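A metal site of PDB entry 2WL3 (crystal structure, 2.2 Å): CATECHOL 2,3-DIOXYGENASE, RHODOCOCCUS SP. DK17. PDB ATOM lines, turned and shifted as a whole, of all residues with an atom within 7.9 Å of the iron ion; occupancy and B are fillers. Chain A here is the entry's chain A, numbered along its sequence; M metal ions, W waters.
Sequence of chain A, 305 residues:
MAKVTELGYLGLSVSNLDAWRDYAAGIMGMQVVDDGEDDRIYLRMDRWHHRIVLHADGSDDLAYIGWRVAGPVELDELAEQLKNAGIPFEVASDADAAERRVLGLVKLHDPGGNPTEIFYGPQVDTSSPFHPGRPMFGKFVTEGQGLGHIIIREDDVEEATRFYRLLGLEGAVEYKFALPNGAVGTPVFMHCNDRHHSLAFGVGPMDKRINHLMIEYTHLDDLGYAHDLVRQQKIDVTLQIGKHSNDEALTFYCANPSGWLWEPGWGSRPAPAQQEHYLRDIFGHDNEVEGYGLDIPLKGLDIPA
OH of Tyr 253 touches the iron ion, 3.1 Å away. The nearest printed residue that does not touch the iron ion is Met 214 (4.2 Å).
The backbone carbonyl oxygen (O) of His 149 is in hydrogen-bond range of the backbone NH (N) of Met 214, at 2.9 Å. The side-chain carboxylate (OE2) of Glu 263 sits at hydrogen-bond distance from the side-chain hydroxyl (OH) of Tyr 253 (3.1 Å). The backbone NH of Glu 263 is in hydrogen-bond range of the backbone carbonyl oxygen of Leu 213. OG1 of Thr 251 lies within hydrogen-bond range of OE2 of Glu 263 (2.9 Å). O of Glu 263 is in hydrogen-bond range of N of Ile 215 (3.3 Å). N of Ile 151 is in hydrogen-bond range of O of His 212 (3.2 Å). A ring nitrogen (ND1) of His 212 lies within hydrogen-bond range of the side-chain amide nitrogen (ND2) of Asn 211 (3.0 Å). The side-chain hydroxyl (OH) of Tyr 253 sits at hydrogen-bond distance from a ring nitrogen (NE2) of His 244, 2.7 Å away.
The iron ion is bound by a ring nitrogen (NE2) of His 149 (2.3 Å), water W1 (2.3 Å), the side-chain carboxylate of Glu 263 (2.3 Å) and a ring nitrogen (NE2) of His 212 (2.5 Å). The iron ion has four donor atoms within binding distance. Slightly farther from the iron ion lies water W2 (2.7 Å).
Water W2 bridges OD2 of Asp 247 and OE2 of Glu 263.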
ATOM      1  N   HIS A 149     -31.161  29.933   4.707  1.00  0.00           N
ATOM      2  CA  HIS A 149     -29.884  30.624   4.878  1.00  0.00           C
ATOM      3  C   HIS A 149     -28.767  30.018   4.051  1.00  0.00           C
ATOM      4  O   HIS A 149     -28.807  28.853   3.709  1.00  0.00           O
ATOM      5  CB  HIS A 149     -29.514  30.778   6.362  1.00  0.00           C
ATOM      6  CG  HIS A 149     -29.088  29.522   7.042  1.00  0.00           C
ATOM      7  ND1 HIS A 149     -29.732  29.018   8.146  1.00  0.00           N
ATOM      8  CD2 HIS A 149     -28.030  28.701   6.815  1.00  0.00           C
ATOM      9  CE1 HIS A 149     -29.120  27.923   8.560  1.00  0.00           C
ATOM     10  NE2 HIS A 149     -28.081  27.707   7.766  1.00  0.00           N
ATOM     11  N   ILE A 150     -27.778  30.831   3.715  1.00  0.00           N
ATOM     12  CA  ILE A 150     -26.700  30.372   2.848  1.00  0.00           C
ATOM     13  C   ILE A 150     -25.349  30.679   3.457  1.00  0.00           C
ATOM     14  O   ILE A 150     -25.208  31.660   4.193  1.00  0.00           O
ATOM     15  CB  ILE A 150     -26.802  30.975   1.427  1.00  0.00           C
ATOM     16  CG1 ILE A 150     -26.835  32.507   1.492  1.00  0.00           C
ATOM     17  CG2 ILE A 150     -28.039  30.423   0.688  1.00  0.00           C
ATOM     18  CD1 ILE A 150     -26.934  33.179   0.147  1.00  0.00           C
ATOM     19  N   ILE A 151     -24.372  29.821   3.183  1.00  0.00           N
ATOM     20  CA  ILE A 151     -22.968  30.102   3.463  1.00  0.00           C
ATOM     21  C   ILE A 151     -22.291  30.389   2.113  1.00  0.00           C
ATOM     22  O   ILE A 151     -22.339  29.563   1.184  1.00  0.00           O
ATOM     23  CB  ILE A 151     -22.248  28.931   4.158  1.00  0.00           C
ATOM     24  CG1 ILE A 151     -22.795  28.714   5.570  1.00  0.00           C
ATOM     25  CG2 ILE A 151     -20.721  29.195   4.271  1.00  0.00           C
ATOM     26  CD1 ILE A 151     -21.903  27.799   6.439  1.00  0.00           C
ATOM     27  N   PHE A 189     -21.981  35.002  11.418  1.00  0.00           N
ATOM     28  CA  PHE A 189     -23.358  34.690  11.078  1.00  0.00           C
ATOM     29  C   PHE A 189     -24.201  35.955  11.140  1.00  0.00           C
ATOM     30  O   PHE A 189     -24.054  36.744  12.068  1.00  0.00           O
ATOM     31  CB  PHE A 189     -23.914  33.629  12.051  1.00  0.00           C
ATOM     32  CG  PHE A 189     -23.501  32.216  11.723  1.00  0.00           C
ATOM     33  CD1 PHE A 189     -24.401  31.330  11.158  1.00  0.00           C
ATOM     34  CD2 PHE A 189     -22.203  31.769  11.996  1.00  0.00           C
ATOM     35  CE1 PHE A 189     -24.023  30.019  10.853  1.00  0.00           C
ATOM     36  CE2 PHE A 189     -21.815  30.454  11.701  1.00  0.00           C
ATOM     37  CZ  PHE A 189     -22.726  29.588  11.133  1.00  0.00           C
ATOM     38  N   HIS A 197     -30.262  33.220  11.276  1.00  0.00           N
ATOM     39  CA  HIS A 197     -29.410  33.928  10.353  1.00  0.00           C
ATOM     40  C   HIS A 197     -29.875  33.615   8.949  1.00  0.00           C
ATOM     41  O   HIS A 197     -30.498  32.561   8.727  1.00  0.00           O
ATOM     42  CB  HIS A 197     -27.934  33.549  10.542  1.00  0.00           C
ATOM     43  CG  HIS A 197     -27.614  32.131  10.191  1.00  0.00           C
ATOM     44  ND1 HIS A 197     -27.820  31.083  11.071  1.00  0.00           N
ATOM     45  CD2 HIS A 197     -27.102  31.577   9.062  1.00  0.00           C
ATOM     46  CE1 HIS A 197     -27.457  29.952  10.493  1.00  0.00           C
ATOM     47  NE2 HIS A 197     -27.012  30.232   9.275  1.00  0.00           N
ATOM     48  N   ALA A 200     -24.124  33.329   6.300  1.00  0.00           N
ATOM     49  CA  ALA A 200     -22.892  33.104   7.066  1.00  0.00           C
ATOM     50  C   ALA A 200     -21.676  33.086   6.146  1.00  0.00           C
ATOM     51  O   ALA A 200     -21.801  32.722   4.970  1.00  0.00           O
ATOM     52  CB  ALA A 200     -22.982  31.813   7.858  1.00  0.00           C
ATOM     53  N   ASN A 211     -21.637  27.160  -0.267  1.00  0.00           N
ATOM     54  CA  ASN A 211     -21.228  25.929   0.441  1.00  0.00           C
ATOM     55  C   ASN A 211     -22.442  25.102   0.743  1.00  0.00           C
ATOM     56  O   ASN A 211     -22.428  23.874   0.574  1.00  0.00           O
ATOM     57  CB  ASN A 211     -20.519  26.264   1.770  1.00  0.00           C
ATOM     58  CG  ASN A 211     -20.349  25.033   2.684  1.00  0.00           C
ATOM     59  OD1 ASN A 211     -19.520  24.161   2.421  1.00  0.00           O
ATOM     60  ND2 ASN A 211     -21.105  25.007   3.775  1.00  0.00           N
ATOM     61  N   HIS A 212     -23.478  25.783   1.220  1.00  0.00           N
ATOM     62  CA  HIS A 212     -24.745  25.134   1.466  1.00  0.00           C
ATOM     63  C   HIS A 212     -25.908  26.114   1.558  1.00  0.00           C
ATOM     64  O   HIS A 212     -25.727  27.332   1.743  1.00  0.00           O
ATOM     65  CB  HIS A 212     -24.682  24.203   2.693  1.00  0.00           C
ATOM     66  CG  HIS A 212     -24.921  24.881   3.989  1.00  0.00           C
ATOM     67  ND1 HIS A 212     -23.898  25.334   4.796  1.00  0.00           N
ATOM     68  CD2 HIS A 212     -26.074  25.179   4.638  1.00  0.00           C
ATOM     69  CE1 HIS A 212     -24.417  25.879   5.886  1.00  0.00           C
ATOM     70  NE2 HIS A 212     -25.728  25.798   5.821  1.00  0.00           N
ATOM     71  N   LEU A 213     -27.106  25.557   1.411  1.00  0.00           N
ATOM     72  CA  LEU A 213     -28.354  26.262   1.641  1.00  0.00           C
ATOM     73  C   LEU A 213     -29.182  25.422   2.614  1.00  0.00           C
ATOM     74  O   LEU A 213     -29.396  24.226   2.388  1.00  0.00           O
ATOM     75  CB  LEU A 213     -29.094  26.444   0.326  1.00  0.00           C
ATOM     76  CG  LEU A 213     -30.613  26.651   0.315  1.00  0.00           C
ATOM     77  CD1 LEU A 213     -30.967  28.039   0.858  1.00  0.00           C
ATOM     78  CD2 LEU A 213     -31.170  26.448  -1.088  1.00  0.00           C
ATOM     79  N   MET A 214     -29.627  26.030   3.706  1.00  0.00           N
ATOM     80  CA  MET A 214     -30.560  25.333   4.569  1.00  0.00           C
ATOM     81  C   MET A 214     -31.963  25.775   4.214  1.00  0.00           C
ATOM     82  O   MET A 214     -32.190  26.943   3.926  1.00  0.00           O
ATOM     83  CB  MET A 214     -30.223  25.560   6.041  1.00  0.00           C
ATOM     84  CG  MET A 214     -31.024  26.628   6.743  1.00  0.00           C
ATOM     85  SD  MET A 214     -32.705  26.057   7.482  1.00  0.00           S
ATOM     86  CE  MET A 214     -32.939  27.463   8.826  1.00  0.00           C
ATOM     87  N   ILE A 215     -32.880  24.828   4.191  1.00  0.00           N
ATOM     88  CA  ILE A 215     -34.297  25.120   3.960  1.00  0.00           C
ATOM     89  C   ILE A 215     -35.061  24.492   5.119  1.00  0.00           C
ATOM     90  O   ILE A 215     -34.647  23.467   5.660  1.00  0.00           O
ATOM     91  CB  ILE A 215     -34.815  24.590   2.610  1.00  0.00           C
ATOM     92  CG1 ILE A 215     -34.451  23.113   2.424  1.00  0.00           C
ATOM     93  CG2 ILE A 215     -34.232  25.426   1.457  1.00  0.00           C
ATOM     94  CD1 ILE A 215     -35.338  22.363   1.402  1.00  0.00           C
ATOM     95  N   HIS A 244     -26.885  22.441  15.623  1.00  0.00           N
ATOM     96  CA  HIS A 244     -25.882  23.480  15.909  1.00  0.00           C
ATOM     97  C   HIS A 244     -26.239  24.285  17.165  1.00  0.00           C
ATOM     98  O   HIS A 244     -27.423  24.496  17.442  1.00  0.00           O
ATOM     99  CB  HIS A 244     -25.775  24.485  14.766  1.00  0.00           C
ATOM    100  CG  HIS A 244     -25.284  23.906  13.469  1.00  0.00           C
ATOM    101  ND1 HIS A 244     -23.968  23.519  13.271  1.00  0.00           N
ATOM    102  CD2 HIS A 244     -25.915  23.703  12.291  1.00  0.00           C
ATOM    103  CE1 HIS A 244     -23.834  23.082  12.042  1.00  0.00           C
ATOM    104  NE2 HIS A 244     -24.999  23.181  11.420  1.00  0.00           N
ATOM    105  N   ASN A 246     -25.810  27.529  17.666  1.00  0.00           N
ATOM    106  CA  ASN A 246     -26.335  28.866  17.395  1.00  0.00           C
ATOM    107  C   ASN A 246     -27.814  28.900  17.031  1.00  0.00           C
ATOM    108  O   ASN A 246     -28.584  29.564  17.711  1.00  0.00           O
ATOM    109  CB  ASN A 246     -25.456  29.659  16.403  1.00  0.00           C
ATOM    110  CG  ASN A 246     -25.274  28.942  15.066  1.00  0.00           C
ATOM    111  OD1 ASN A 246     -25.681  27.806  14.884  1.00  0.00           O
ATOM    112  ND2 ASN A 246     -24.643  29.641  14.125  1.00  0.00           N
ATOM    113  N   ASP A 247     -28.204  28.172  15.989  1.00  0.00           N
ATOM    114  CA  ASP A 247     -29.590  28.179  15.538  1.00  0.00           C
ATOM    115  C   ASP A 247     -30.465  27.164  16.281  1.00  0.00           C
ATOM    116  O   ASP A 247     -31.692  27.274  16.256  1.00  0.00           O
ATOM    117  CB  ASP A 247     -29.688  27.984  14.011  1.00  0.00           C
ATOM    118  CG  ASP A 247     -29.166  26.633  13.551  1.00  0.00           C
ATOM    119  OD1 ASP A 247     -28.909  25.744  14.394  1.00  0.00           O
ATOM    120  OD2 ASP A 247     -29.004  26.461  12.313  1.00  0.00           O
ATOM    121  N   ALA A 249     -31.317  24.258  15.485  1.00  0.00           N
ATOM    122  CA  ALA A 249     -32.215  23.607  14.525  1.00  0.00           C
ATOM    123  C   ALA A 249     -31.876  22.146  14.360  1.00  0.00           C
ATOM    124  O   ALA A 249     -30.709  21.777  14.450  1.00  0.00           O
ATOM    125  CB  ALA A 249     -32.143  24.304  13.171  1.00  0.00           C
ATOM    126  N   THR A 251     -31.257  19.300  11.850  1.00  0.00           N
ATOM    127  CA  THR A 251     -30.875  19.269  10.427  1.00  0.00           C
ATOM    128  C   THR A 251     -29.952  18.128  10.003  1.00  0.00           C
ATOM    129  O   THR A 251     -29.215  17.568  10.836  1.00  0.00           O
ATOM    130  CB  THR A 251     -30.152  20.576   9.989  1.00  0.00           C
ATOM    131  OG1 THR A 251     -28.828  20.602  10.537  1.00  0.00           O
ATOM    132  CG2 THR A 251     -30.904  21.841  10.390  1.00  0.00           C
ATOM    133  N   TYR A 253     -27.144  17.368   6.421  1.00  0.00           N
ATOM    134  CA  TYR A 253     -26.455  18.014   5.294  1.00  0.00           C
ATOM    135  C   TYR A 253     -26.228  17.024   4.152  1.00  0.00           C
ATOM    136  O   TYR A 253     -25.424  16.100   4.306  1.00  0.00           O
ATOM    137  CB  TYR A 253     -25.095  18.548   5.761  1.00  0.00           C
ATOM    138  CG  TYR A 253     -25.070  19.853   6.554  1.00  0.00           C
ATOM    139  CD1 TYR A 253     -24.673  21.049   5.945  1.00  0.00           C
ATOM    140  CD2 TYR A 253     -25.415  19.884   7.916  1.00  0.00           C
ATOM    141  CE1 TYR A 253     -24.639  22.267   6.674  1.00  0.00           C
ATOM    142  CE2 TYR A 253     -25.382  21.067   8.654  1.00  0.00           C
ATOM    143  CZ  TYR A 253     -24.995  22.267   8.036  1.00  0.00           C
ATOM    144  OH  TYR A 253     -24.966  23.446   8.754  1.00  0.00           O
ATOM    145  N   GLU A 263     -29.238  21.618   3.207  1.00  0.00           N
ATOM    146  CA  GLU A 263     -29.398  21.264   4.618  1.00  0.00           C
ATOM    147  C   GLU A 263     -30.872  21.377   5.020  1.00  0.00           C
ATOM    148  O   GLU A 263     -31.246  22.344   5.661  1.00  0.00           O
ATOM    149  CB  GLU A 263     -28.513  22.161   5.509  1.00  0.00           C
ATOM    150  CG  GLU A 263     -28.694  21.976   7.040  1.00  0.00           C
ATOM    151  CD  GLU A 263     -28.181  23.144   7.896  1.00  0.00           C
ATOM    152  OE1 GLU A 263     -27.940  24.251   7.361  1.00  0.00           O
ATOM    153  OE2 GLU A 263     -28.002  22.954   9.114  1.00  0.00           O
ATOM    154  N   HIS A 285     -24.520  15.933  14.066  1.00  0.00           N
ATOM    155  CA  HIS A 285     -23.821  16.559  12.942  1.00  0.00           C
ATOM    156  C   HIS A 285     -22.504  15.864  12.570  1.00  0.00           C
ATOM    157  O   HIS A 285     -21.643  16.449  11.916  1.00  0.00           O
ATOM    158  CB  HIS A 285     -23.577  18.055  13.181  1.00  0.00           C
ATOM    159  CG  HIS A 285     -24.776  18.910  12.892  1.00  0.00           C
ATOM    160  ND1 HIS A 285     -25.718  18.564  11.948  1.00  0.00           N
ATOM    161  CD2 HIS A 285     -25.167  20.103  13.407  1.00  0.00           C
ATOM    162  CE1 HIS A 285     -26.645  19.508  11.908  1.00  0.00           C
ATOM    163  NE2 HIS A 285     -26.337  20.442  12.779  1.00  0.00           N
HETATM  164 FE    FE M   1     -26.574  26.005   8.111  1.00  0.00          FE
HETATM  165  O   HOH W   1     -25.106  27.628   8.925  1.00  0.00           O
HETATM  166  O   HOH W   2     -28.043  25.319  10.317  1.00  0.00           O
